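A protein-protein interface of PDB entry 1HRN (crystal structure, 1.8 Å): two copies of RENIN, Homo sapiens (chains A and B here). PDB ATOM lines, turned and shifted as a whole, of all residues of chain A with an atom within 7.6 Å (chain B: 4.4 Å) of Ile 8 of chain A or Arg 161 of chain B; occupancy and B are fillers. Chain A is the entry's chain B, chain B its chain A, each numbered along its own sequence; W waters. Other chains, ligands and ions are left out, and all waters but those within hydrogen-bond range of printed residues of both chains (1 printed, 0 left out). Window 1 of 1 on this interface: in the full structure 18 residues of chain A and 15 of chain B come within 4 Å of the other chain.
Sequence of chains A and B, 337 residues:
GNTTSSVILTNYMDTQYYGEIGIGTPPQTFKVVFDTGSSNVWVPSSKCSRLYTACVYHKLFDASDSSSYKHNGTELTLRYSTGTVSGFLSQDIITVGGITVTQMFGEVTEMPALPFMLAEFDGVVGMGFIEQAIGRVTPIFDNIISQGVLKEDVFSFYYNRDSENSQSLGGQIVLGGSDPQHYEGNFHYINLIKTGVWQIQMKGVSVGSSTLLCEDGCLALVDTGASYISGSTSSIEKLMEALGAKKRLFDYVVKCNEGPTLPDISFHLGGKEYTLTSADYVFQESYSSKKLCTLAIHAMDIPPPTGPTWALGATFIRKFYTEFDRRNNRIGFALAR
The side-chain amino group (NZ) of Lys 319 of chain B lies within salt-bridge range of the side-chain carboxylate (OE1) of Glu 20 of chain A.
The side-chain amide oxygen of Asn 11 of chain B sits at hydrogen-bond distance from the backbone NH of Asp 162 of chain B, at 3.4 Å. The side-chain amino group (NZ) of Lys 319 of chain B lies within salt-bridge range of the side-chain carboxylate (OD2) of Asp 280 of chain B, at 3.2 Å. The guanidinium group (NH2) of Arg 161 of chain B is in salt-bridge range of the side-chain carboxylate (OD1) of Asp 280 of chain B (3.4 Å). N of Asp 162 of chain B lies within hydrogen-bond range of OD1 of Asp 14 of chain B (3.0 Å). NH1 of Arg 161 of chain B is in hydrogen-bond range of O of Arg 318 of chain B, at 3.3 Å.
Among the printed residues, pairs that only touch across the chains: Ile 8 of chain A with Arg 161 of chain B (3.8 Å), Glu 20 of chain A with Asp 280 of chain B (3.7 Å) and Ser 168 of chain A with Asp 162 of chain B (3.3 Å).
Of chain B, only Arg 161 (3.8 Å) comes within 4 Å of Ile 8 of chain A. Leu 9 of chain A touches none of the printed residues of chain B. Asn 11 of chain A touches none of the printed residues of chain B. Printed residues of chain B within 4 Å of Ser 168 of chain A: Asp 162. Arg 161 of chain B touches just one residue of chain A: Ile 8 (3.8 Å). Printed residues of chain A within 4 Å of Asp 162 of chain B: Ser 168 (3.3 Å).
Printed residues of chain A that touch a printed residue of chain B: Ile 8, Glu 20 and Ser 168. Hydrophobic or aromatic side chains of chain A within 4 Å of the printed part of chain B: Ile 8. Of the 10 printed residues of chain B, 4 touch a printed residue of chain A. Among the printed residues, 4 pairs touch across the chains. Among the printed residues, Asp or Glu carboxylates within 4 Å of a Lys or Arg side-chain nitrogen of the other chain: Glu 20 of chain A with Lys 319 of chain B (2.7 Å).
Position printed for both chains: 11.
Water W1 lies within hydrogen-bond range of the backbone NH of Leu 169 of chain A and the backbone carbonyl oxygen of Asp 162 of chain B.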
ATOM      1  N   SER A   6       8.739   0.101  -7.989  1.00  0.00           N
ATOM      2  CA  SER A   6       8.679   1.478  -7.500  1.00  0.00           C
ATOM      3  C   SER A   6       9.057   2.485  -8.566  1.00  0.00           C
ATOM      4  O   SER A   6       9.720   2.138  -9.555  1.00  0.00           O
ATOM      5  CB  SER A   6       9.584   1.666  -6.328  1.00  0.00           C
ATOM      6  OG  SER A   6      10.841   1.153  -6.634  1.00  0.00           O
ATOM      7  N   VAL A   7       8.626   3.733  -8.351  1.00  0.00           N
ATOM      8  CA  VAL A   7       8.877   4.840  -9.302  1.00  0.00           C
ATOM      9  C   VAL A   7       9.428   5.999  -8.526  1.00  0.00           C
ATOM     10  O   VAL A   7       8.758   6.477  -7.627  1.00  0.00           O
ATOM     11  CB  VAL A   7       7.581   5.264 -10.059  1.00  0.00           C
ATOM     12  CG1 VAL A   7       7.874   6.361 -11.087  1.00  0.00           C
ATOM     13  CG2 VAL A   7       6.966   4.062 -10.773  1.00  0.00           C
ATOM     14  N   ILE A   8      10.613   6.448  -8.828  1.00  0.00           N
ATOM     15  CA  ILE A   8      11.194   7.550  -8.084  1.00  0.00           C
ATOM     16  C   ILE A   8      10.527   8.796  -8.558  1.00  0.00           C
ATOM     17  O   ILE A   8      10.326   8.902  -9.748  1.00  0.00           O
ATOM     18  CB  ILE A   8      12.633   7.640  -8.437  1.00  0.00           C
ATOM     19  CG1 ILE A   8      13.268   6.378  -7.914  1.00  0.00           C
ATOM     20  CG2 ILE A   8      13.256   8.802  -7.705  1.00  0.00           C
ATOM     21  CD1 ILE A   8      12.933   6.177  -6.447  1.00  0.00           C
ATOM     22  N   LEU A   9      10.156   9.715  -7.673  1.00  0.00           N
ATOM     23  CA  LEU A   9       9.489  10.893  -8.141  1.00  0.00           C
ATOM     24  C   LEU A   9      10.388  12.115  -7.996  1.00  0.00           C
ATOM     25  O   LEU A   9      11.290  12.138  -7.149  1.00  0.00           O
ATOM     26  CB  LEU A   9       8.101  11.169  -7.431  1.00  0.00           C
ATOM     27  CG  LEU A   9       7.139   9.980  -7.258  1.00  0.00           C
ATOM     28  CD1 LEU A   9       5.967  10.336  -6.315  1.00  0.00           C
ATOM     29  CD2 LEU A   9       6.628   9.512  -8.620  1.00  0.00           C
ATOM     30  N   THR A  10      10.057  13.151  -8.806  1.00  0.00           N
ATOM     31  CA  THR A  10      10.645  14.475  -8.714  1.00  0.00           C
ATOM     32  C   THR A  10       9.653  15.339  -7.980  1.00  0.00           C
ATOM     33  O   THR A  10       8.458  15.202  -8.125  1.00  0.00           O
ATOM     34  CB  THR A  10      10.963  15.130 -10.088  1.00  0.00           C
ATOM     35  OG1 THR A  10      12.027  14.449 -10.703  1.00  0.00           O
ATOM     36  CG2 THR A  10      11.378  16.597  -9.954  1.00  0.00           C
ATOM     37  N   ASN A  11      10.173  16.141  -7.099  1.00  0.00           N
ATOM     38  CA  ASN A  11       9.397  17.056  -6.275  1.00  0.00           C
ATOM     39  C   ASN A  11       9.741  18.448  -6.795  1.00  0.00           C
ATOM     40  O   ASN A  11      10.862  18.957  -6.589  1.00  0.00           O
ATOM     41  CB  ASN A  11       9.789  16.959  -4.761  1.00  0.00           C
ATOM     42  CG  ASN A  11       9.296  18.044  -3.814  1.00  0.00           C
ATOM     43  OD1 ASN A  11       9.487  17.995  -2.604  1.00  0.00           O
ATOM     44  ND2 ASN A  11       8.617  19.022  -4.341  1.00  0.00           N
ATOM     45  N   TYR A  18       6.125  14.077  -9.702  1.00  0.00           N
ATOM     46  CA  TYR A  18       5.849  13.289 -10.870  1.00  0.00           C
ATOM     47  C   TYR A  18       6.917  12.299 -11.134  1.00  0.00           C
ATOM     48  O   TYR A  18       8.035  12.470 -10.696  1.00  0.00           O
ATOM     49  CB  TYR A  18       5.652  14.228 -12.085  1.00  0.00           C
ATOM     50  CG  TYR A  18       6.639  15.342 -12.067  1.00  0.00           C
ATOM     51  CD1 TYR A  18       6.363  16.519 -11.387  1.00  0.00           C
ATOM     52  CD2 TYR A  18       7.834  15.259 -12.761  1.00  0.00           C
ATOM     53  CE1 TYR A  18       7.321  17.524 -11.317  1.00  0.00           C
ATOM     54  CE2 TYR A  18       8.763  16.302 -12.790  1.00  0.00           C
ATOM     55  CZ  TYR A  18       8.537  17.414 -11.987  1.00  0.00           C
ATOM     56  OH  TYR A  18       9.471  18.445 -11.931  1.00  0.00           O
ATOM     57  N   GLY A  19       6.594  11.262 -11.874  1.00  0.00           N
ATOM     58  CA  GLY A  19       7.592  10.261 -12.192  1.00  0.00           C
ATOM     59  C   GLY A  19       7.549   9.860 -13.653  1.00  0.00           C
ATOM     60  O   GLY A  19       6.768  10.421 -14.420  1.00  0.00           O
ATOM     61  N   GLU A  20       8.416   8.930 -14.039  1.00  0.00           N
ATOM     62  CA  GLU A  20       8.520   8.487 -15.430  1.00  0.00           C
ATOM     63  C   GLU A  20       7.702   7.256 -15.761  1.00  0.00           C
ATOM     64  O   GLU A  20       7.626   6.307 -15.018  1.00  0.00           O
ATOM     65  CB  GLU A  20       9.958   8.136 -15.867  1.00  0.00           C
ATOM     66  CG  GLU A  20      10.996   9.301 -15.977  1.00  0.00           C
ATOM     67  CD  GLU A  20      12.506   8.866 -15.886  1.00  0.00           C
ATOM     68  OE1 GLU A  20      13.082   8.070 -16.697  1.00  0.00           O
ATOM     69  OE2 GLU A  20      13.175   9.476 -14.883  1.00  0.00           O
ATOM     70  N   VAL A  32       4.758  11.786 -15.387  1.00  0.00           N
ATOM     71  CA  VAL A  32       3.347  11.765 -15.032  1.00  0.00           C
ATOM     72  C   VAL A  32       3.108  12.005 -13.535  1.00  0.00           C
ATOM     73  O   VAL A  32       3.941  11.657 -12.661  1.00  0.00           O
ATOM     74  CB  VAL A  32       2.624  10.483 -15.506  1.00  0.00           C
ATOM     75  CG1 VAL A  32       2.366  10.520 -17.018  1.00  0.00           C
ATOM     76  CG2 VAL A  32       3.463   9.283 -15.173  1.00  0.00           C
ATOM     77  N   PHE A  34       0.936  10.735 -10.451  1.00  0.00           N
ATOM     78  CA  PHE A  34       0.164   9.553 -10.179  1.00  0.00           C
ATOM     79  C   PHE A  34      -0.902  10.043  -9.226  1.00  0.00           C
ATOM     80  O   PHE A  34      -0.578  10.433  -8.111  1.00  0.00           O
ATOM     81  CB  PHE A  34       1.040   8.462  -9.579  1.00  0.00           C
ATOM     82  CG  PHE A  34       2.075   7.919 -10.546  1.00  0.00           C
ATOM     83  CD1 PHE A  34       3.281   8.589 -10.757  1.00  0.00           C
ATOM     84  CD2 PHE A  34       1.896   6.705 -11.210  1.00  0.00           C
ATOM     85  CE1 PHE A  34       4.265   8.086 -11.611  1.00  0.00           C
ATOM     86  CE2 PHE A  34       2.894   6.129 -11.993  1.00  0.00           C
ATOM     87  CZ  PHE A  34       4.065   6.848 -12.222  1.00  0.00           C
ATOM     88  N   GLY A  97       8.064   1.607 -13.672  1.00  0.00           N
ATOM     89  CA  GLY A  97       9.042   0.945 -12.870  1.00  0.00           C
ATOM     90  C   GLY A  97       9.431  -0.358 -13.571  1.00  0.00           C
ATOM     91  O   GLY A  97       9.751  -0.365 -14.732  1.00  0.00           O
ATOM     92  N   TYR A 158       5.211   8.047  -1.056  1.00  0.00           N
ATOM     93  CA  TYR A 158       6.150   8.775  -0.228  1.00  0.00           C
ATOM     94  C   TYR A 158       6.351  10.090  -0.949  1.00  0.00           C
ATOM     95  O   TYR A 158       6.760  10.123  -2.122  1.00  0.00           O
ATOM     96  CB  TYR A 158       7.518   7.994  -0.053  1.00  0.00           C
ATOM     97  CG  TYR A 158       8.599   8.861   0.600  1.00  0.00           C
ATOM     98  CD1 TYR A 158       8.426   9.363   1.898  1.00  0.00           C
ATOM     99  CD2 TYR A 158       9.735   9.244  -0.116  1.00  0.00           C
ATOM    100  CE1 TYR A 158       9.343  10.228   2.484  1.00  0.00           C
ATOM    101  CE2 TYR A 158      10.647  10.144   0.444  1.00  0.00           C
ATOM    102  CZ  TYR A 158      10.472  10.608   1.754  1.00  0.00           C
ATOM    103  OH  TYR A 158      11.342  11.519   2.291  1.00  0.00           O
ATOM    104  N   SER A 168      18.119  14.496  -2.741  1.00  0.00           N
ATOM    105  CA  SER A 168      17.291  13.445  -2.161  1.00  0.00           C
ATOM    106  C   SER A 168      16.285  13.069  -3.179  1.00  0.00           C
ATOM    107  O   SER A 168      15.994  13.939  -4.032  1.00  0.00           O
ATOM    108  CB  SER A 168      16.445  13.924  -0.985  1.00  0.00           C
ATOM    109  OG  SER A 168      17.169  14.853  -0.257  1.00  0.00           O
ATOM    110  N   LEU A 169      15.709  11.852  -3.023  1.00  0.00           N
ATOM    111  CA  LEU A 169      14.609  11.513  -3.899  1.00  0.00           C
ATOM    112  C   LEU A 169      13.480  12.503  -3.574  1.00  0.00           C
ATOM    113  O   LEU A 169      13.376  13.004  -2.443  1.00  0.00           O
ATOM    114  CB  LEU A 169      14.161  10.002  -3.925  1.00  0.00           C
ATOM    115  CG  LEU A 169      13.315   9.656  -2.717  1.00  0.00           C
ATOM    116  CD1 LEU A 169      13.163   8.156  -2.490  1.00  0.00           C
ATOM    117  CD2 LEU A 169      13.995  10.260  -1.497  1.00  0.00           C
ATOM    118  N   GLY A 170      12.692  12.862  -4.569  1.00  0.00           N
ATOM    119  CA  GLY A 170      11.622  13.804  -4.330  1.00  0.00           C
ATOM    120  C   GLY A 170      10.401  13.121  -3.728  1.00  0.00           C
ATOM    121  O   GLY A 170       9.528  13.732  -3.133  1.00  0.00           O
ATOM    122  N   GLY A 171      10.334  11.808  -3.981  1.00  0.00           N
ATOM    123  CA  GLY A 171       9.259  10.917  -3.526  1.00  0.00           C
ATOM    124  C   GLY A 171       9.448   9.547  -4.165  1.00  0.00           C
ATOM    125  O   GLY A 171      10.405   9.289  -4.932  1.00  0.00           O
ATOM    126  N   GLN A 172       8.523   8.658  -3.841  1.00  0.00           N
ATOM    127  CA  GLN A 172       8.504   7.304  -4.332  1.00  0.00           C
ATOM    128  C   GLN A 172       7.096   6.662  -4.230  1.00  0.00           C
ATOM    129  O   GLN A 172       6.389   6.766  -3.229  1.00  0.00           O
ATOM    130  CB  GLN A 172       9.570   6.500  -3.559  1.00  0.00           C
ATOM    131  CG  GLN A 172       9.630   4.995  -3.843  1.00  0.00           C
ATOM    132  CD  GLN A 172      10.231   4.178  -2.715  1.00  0.00           C
ATOM    133  OE1 GLN A 172       9.574   3.994  -1.682  1.00  0.00           O
ATOM    134  NE2 GLN A 172      11.460   3.698  -2.883  1.00  0.00           N
ATOM    135  N   ILE A 173       6.702   5.959  -5.290  1.00  0.00           N
ATOM    136  CA  ILE A 173       5.540   5.127  -5.246  1.00  0.00           C
ATOM    137  C   ILE A 173       6.028   3.736  -5.339  1.00  0.00           C
ATOM    138  O   ILE A 173       6.955   3.472  -6.114  1.00  0.00           O
ATOM    139  CB  ILE A 173       4.696   5.289  -6.445  1.00  0.00           C
ATOM    140  CG1 ILE A 173       4.259   6.714  -6.486  1.00  0.00           C
ATOM    141  CG2 ILE A 173       3.487   4.352  -6.382  1.00  0.00           C
ATOM    142  CD1 ILE A 173       3.484   6.857  -7.786  1.00  0.00           C
ATOM    143  N   HIS A 182      11.010   4.507   4.416  1.00  0.00           N
ATOM    144  CA  HIS A 182      10.303   5.801   4.335  1.00  0.00           C
ATOM    145  C   HIS A 182       9.181   6.088   5.315  1.00  0.00           C
ATOM    146  O   HIS A 182       8.534   7.111   5.205  1.00  0.00           O
ATOM    147  CB  HIS A 182       9.867   6.096   2.910  1.00  0.00           C
ATOM    148  CG  HIS A 182      11.090   6.455   2.171  1.00  0.00           C
ATOM    149  ND1 HIS A 182      11.468   5.773   1.006  1.00  0.00           N
ATOM    150  CD2 HIS A 182      12.024   7.376   2.484  1.00  0.00           C
ATOM    151  CE1 HIS A 182      12.636   6.316   0.634  1.00  0.00           C
ATOM    152  NE2 HIS A 182      12.978   7.289   1.495  1.00  0.00           N
ATOM    153  N   ASN B  11      28.008   8.347   0.116  1.00  0.00           N
ATOM    154  CA  ASN B  11      27.743   9.311  -0.932  1.00  0.00           C
ATOM    155  C   ASN B  11      27.979  10.724  -0.388  1.00  0.00           C
ATOM    156  O   ASN B  11      27.103  11.313   0.275  1.00  0.00           O
ATOM    157  CB  ASN B  11      26.264   9.280  -1.422  1.00  0.00           C
ATOM    158  CG  ASN B  11      25.882  10.311  -2.448  1.00  0.00           C
ATOM    159  OD1 ASN B  11      24.769  10.290  -2.989  1.00  0.00           O
ATOM    160  ND2 ASN B  11      26.811  11.173  -2.811  1.00  0.00           N
ATOM    161  N   ASP B  14      26.838  13.667  -3.990  1.00  0.00           N
ATOM    162  CA  ASP B  14      26.522  13.084  -5.295  1.00  0.00           C
ATOM    163  C   ASP B  14      27.700  13.015  -6.299  1.00  0.00           C
ATOM    164  O   ASP B  14      27.510  12.704  -7.482  1.00  0.00           O
ATOM    165  CB  ASP B  14      25.386  13.878  -5.910  1.00  0.00           C
ATOM    166  CG  ASP B  14      24.118  13.162  -5.721  1.00  0.00           C
ATOM    167  OD1 ASP B  14      23.965  12.197  -4.997  1.00  0.00           O
ATOM    168  OD2 ASP B  14      23.211  13.683  -6.397  1.00  0.00           O
ATOM    169  N   TYR B 159      24.421   3.236  -6.737  1.00  0.00           N
ATOM    170  CA  TYR B 159      24.771   4.575  -6.238  1.00  0.00           C
ATOM    171  C   TYR B 159      23.460   5.261  -5.882  1.00  0.00           C
ATOM    172  O   TYR B 159      22.590   5.429  -6.762  1.00  0.00           O
ATOM    173  CB  TYR B 159      25.457   5.466  -7.320  1.00  0.00           C
ATOM    174  CG  TYR B 159      26.921   5.233  -7.507  1.00  0.00           C
ATOM    175  CD1 TYR B 159      27.598   4.342  -6.677  1.00  0.00           C
ATOM    176  CD2 TYR B 159      27.608   5.827  -8.559  1.00  0.00           C
ATOM    177  CE1 TYR B 159      28.976   4.128  -6.787  1.00  0.00           C
ATOM    178  CE2 TYR B 159      28.995   5.640  -8.689  1.00  0.00           C
ATOM    179  CZ  TYR B 159      29.669   4.808  -7.793  1.00  0.00           C
ATOM    180  OH  TYR B 159      31.010   4.666  -7.880  1.00  0.00           O
ATOM    181  N   ASN B 160      23.302   5.693  -4.631  1.00  0.00           N
ATOM    182  CA  ASN B 160      22.054   6.336  -4.269  1.00  0.00           C
ATOM    183  C   ASN B 160      22.036   7.776  -4.596  1.00  0.00           C
ATOM    184  O   ASN B 160      23.062   8.382  -4.776  1.00  0.00           O
ATOM    185  CB  ASN B 160      21.916   6.231  -2.734  1.00  0.00           C
ATOM    186  CG  ASN B 160      20.471   6.348  -2.214  1.00  0.00           C
ATOM    187  OD1 ASN B 160      20.201   6.079  -0.993  1.00  0.00           O
ATOM    188  ND2 ASN B 160      19.579   6.787  -3.085  1.00  0.00           N
ATOM    189  N   ARG B 161      20.888   8.331  -4.548  1.00  0.00           N
ATOM    190  CA  ARG B 161      20.750   9.759  -4.548  1.00  0.00           C
ATOM    191  C   ARG B 161      21.214  10.308  -3.182  1.00  0.00           C
ATOM    192  O   ARG B 161      21.219   9.691  -2.108  1.00  0.00           O
ATOM    193  CB  ARG B 161      19.319  10.217  -4.701  1.00  0.00           C
ATOM    194  CG  ARG B 161      18.906  10.366  -6.150  1.00  0.00           C
ATOM    195  CD  ARG B 161      18.206   9.158  -6.735  1.00  0.00           C
ATOM    196  NE  ARG B 161      17.355   9.519  -7.895  1.00  0.00           N
ATOM    197  CZ  ARG B 161      17.086   8.747  -8.947  1.00  0.00           C
ATOM    198  NH1 ARG B 161      17.545   7.511  -9.067  1.00  0.00           N
ATOM    199  NH2 ARG B 161      16.290   9.233  -9.895  1.00  0.00           N
ATOM    200  N   ASP B 162      21.657  11.520  -3.173  1.00  0.00           N
ATOM    201  CA  ASP B 162      22.118  12.062  -1.916  1.00  0.00           C
ATOM    202  C   ASP B 162      20.983  12.045  -0.888  1.00  0.00           C
ATOM    203  O   ASP B 162      19.829  11.694  -1.125  1.00  0.00           O
ATOM    204  CB  ASP B 162      22.579  13.532  -2.146  1.00  0.00           C
ATOM    205  CG  ASP B 162      23.649  14.018  -1.230  1.00  0.00           C
ATOM    206  OD1 ASP B 162      23.962  13.471  -0.167  1.00  0.00           O
ATOM    207  OD2 ASP B 162      24.161  15.149  -1.668  1.00  0.00           O
ATOM    208  N   SER B 163      21.340  12.460   0.308  1.00  0.00           N
ATOM    209  CA  SER B 163      20.391  12.477   1.385  1.00  0.00           C
ATOM    210  C   SER B 163      20.712  13.510   2.424  1.00  0.00           C
ATOM    211  O   SER B 163      21.866  13.944   2.573  1.00  0.00           O
ATOM    212  CB  SER B 163      20.086  11.124   2.013  1.00  0.00           C
ATOM    213  OG  SER B 163      19.200  11.306   3.129  1.00  0.00           O
ATOM    214  N   ASP B 280      17.530  14.379 -13.207  1.00  0.00           N
ATOM    215  CA  ASP B 280      18.661  13.478 -13.110  1.00  0.00           C
ATOM    216  C   ASP B 280      19.980  14.172 -13.437  1.00  0.00           C
ATOM    217  O   ASP B 280      21.020  13.698 -13.064  1.00  0.00           O
ATOM    218  CB  ASP B 280      18.513  12.230 -14.058  1.00  0.00           C
ATOM    219  CG  ASP B 280      17.237  11.446 -13.890  1.00  0.00           C
ATOM    220  OD1 ASP B 280      16.911  11.183 -12.658  1.00  0.00           O
ATOM    221  OD2 ASP B 280      16.567  11.057 -14.809  1.00  0.00           O
ATOM    222  N   ARG B 318      23.399   6.343 -11.002  1.00  0.00           N
ATOM    223  CA  ARG B 318      22.366   6.564 -10.013  1.00  0.00           C
ATOM    224  C   ARG B 318      21.039   6.055 -10.513  1.00  0.00           C
ATOM    225  O   ARG B 318      20.163   5.689  -9.760  1.00  0.00           O
ATOM    226  CB  ARG B 318      22.192   8.076  -9.736  1.00  0.00           C
ATOM    227  CG  ARG B 318      23.223   8.621  -8.743  1.00  0.00           C
ATOM    228  CD  ARG B 318      22.879   9.975  -8.186  1.00  0.00           C
ATOM    229  NE  ARG B 318      23.204  11.049  -9.108  1.00  0.00           N
ATOM    230  CZ  ARG B 318      24.399  11.656  -9.145  1.00  0.00           C
ATOM    231  NH1 ARG B 318      25.415  11.301  -8.363  1.00  0.00           N
ATOM    232  NH2 ARG B 318      24.540  12.663  -9.971  1.00  0.00           N
ATOM    233  N   LYS B 319      20.826   6.148 -11.807  1.00  0.00           N
ATOM    234  CA  LYS B 319      19.554   5.803 -12.359  1.00  0.00           C
ATOM    235  C   LYS B 319      19.553   4.361 -12.833  1.00  0.00           C
ATOM    236  O   LYS B 319      18.559   3.641 -12.666  1.00  0.00           O
ATOM    237  CB  LYS B 319      19.235   6.825 -13.420  1.00  0.00           C
ATOM    238  CG  LYS B 319      18.166   6.394 -14.329  1.00  0.00           C
ATOM    239  CD  LYS B 319      16.833   6.881 -13.935  1.00  0.00           C
ATOM    240  CE  LYS B 319      15.913   6.829 -15.131  1.00  0.00           C
ATOM    241  NZ  LYS B 319      15.619   8.179 -15.702  1.00  0.00           N
HETATM  242  O   HOH W   1      17.174   9.871  -2.027  1.00  0.00           O
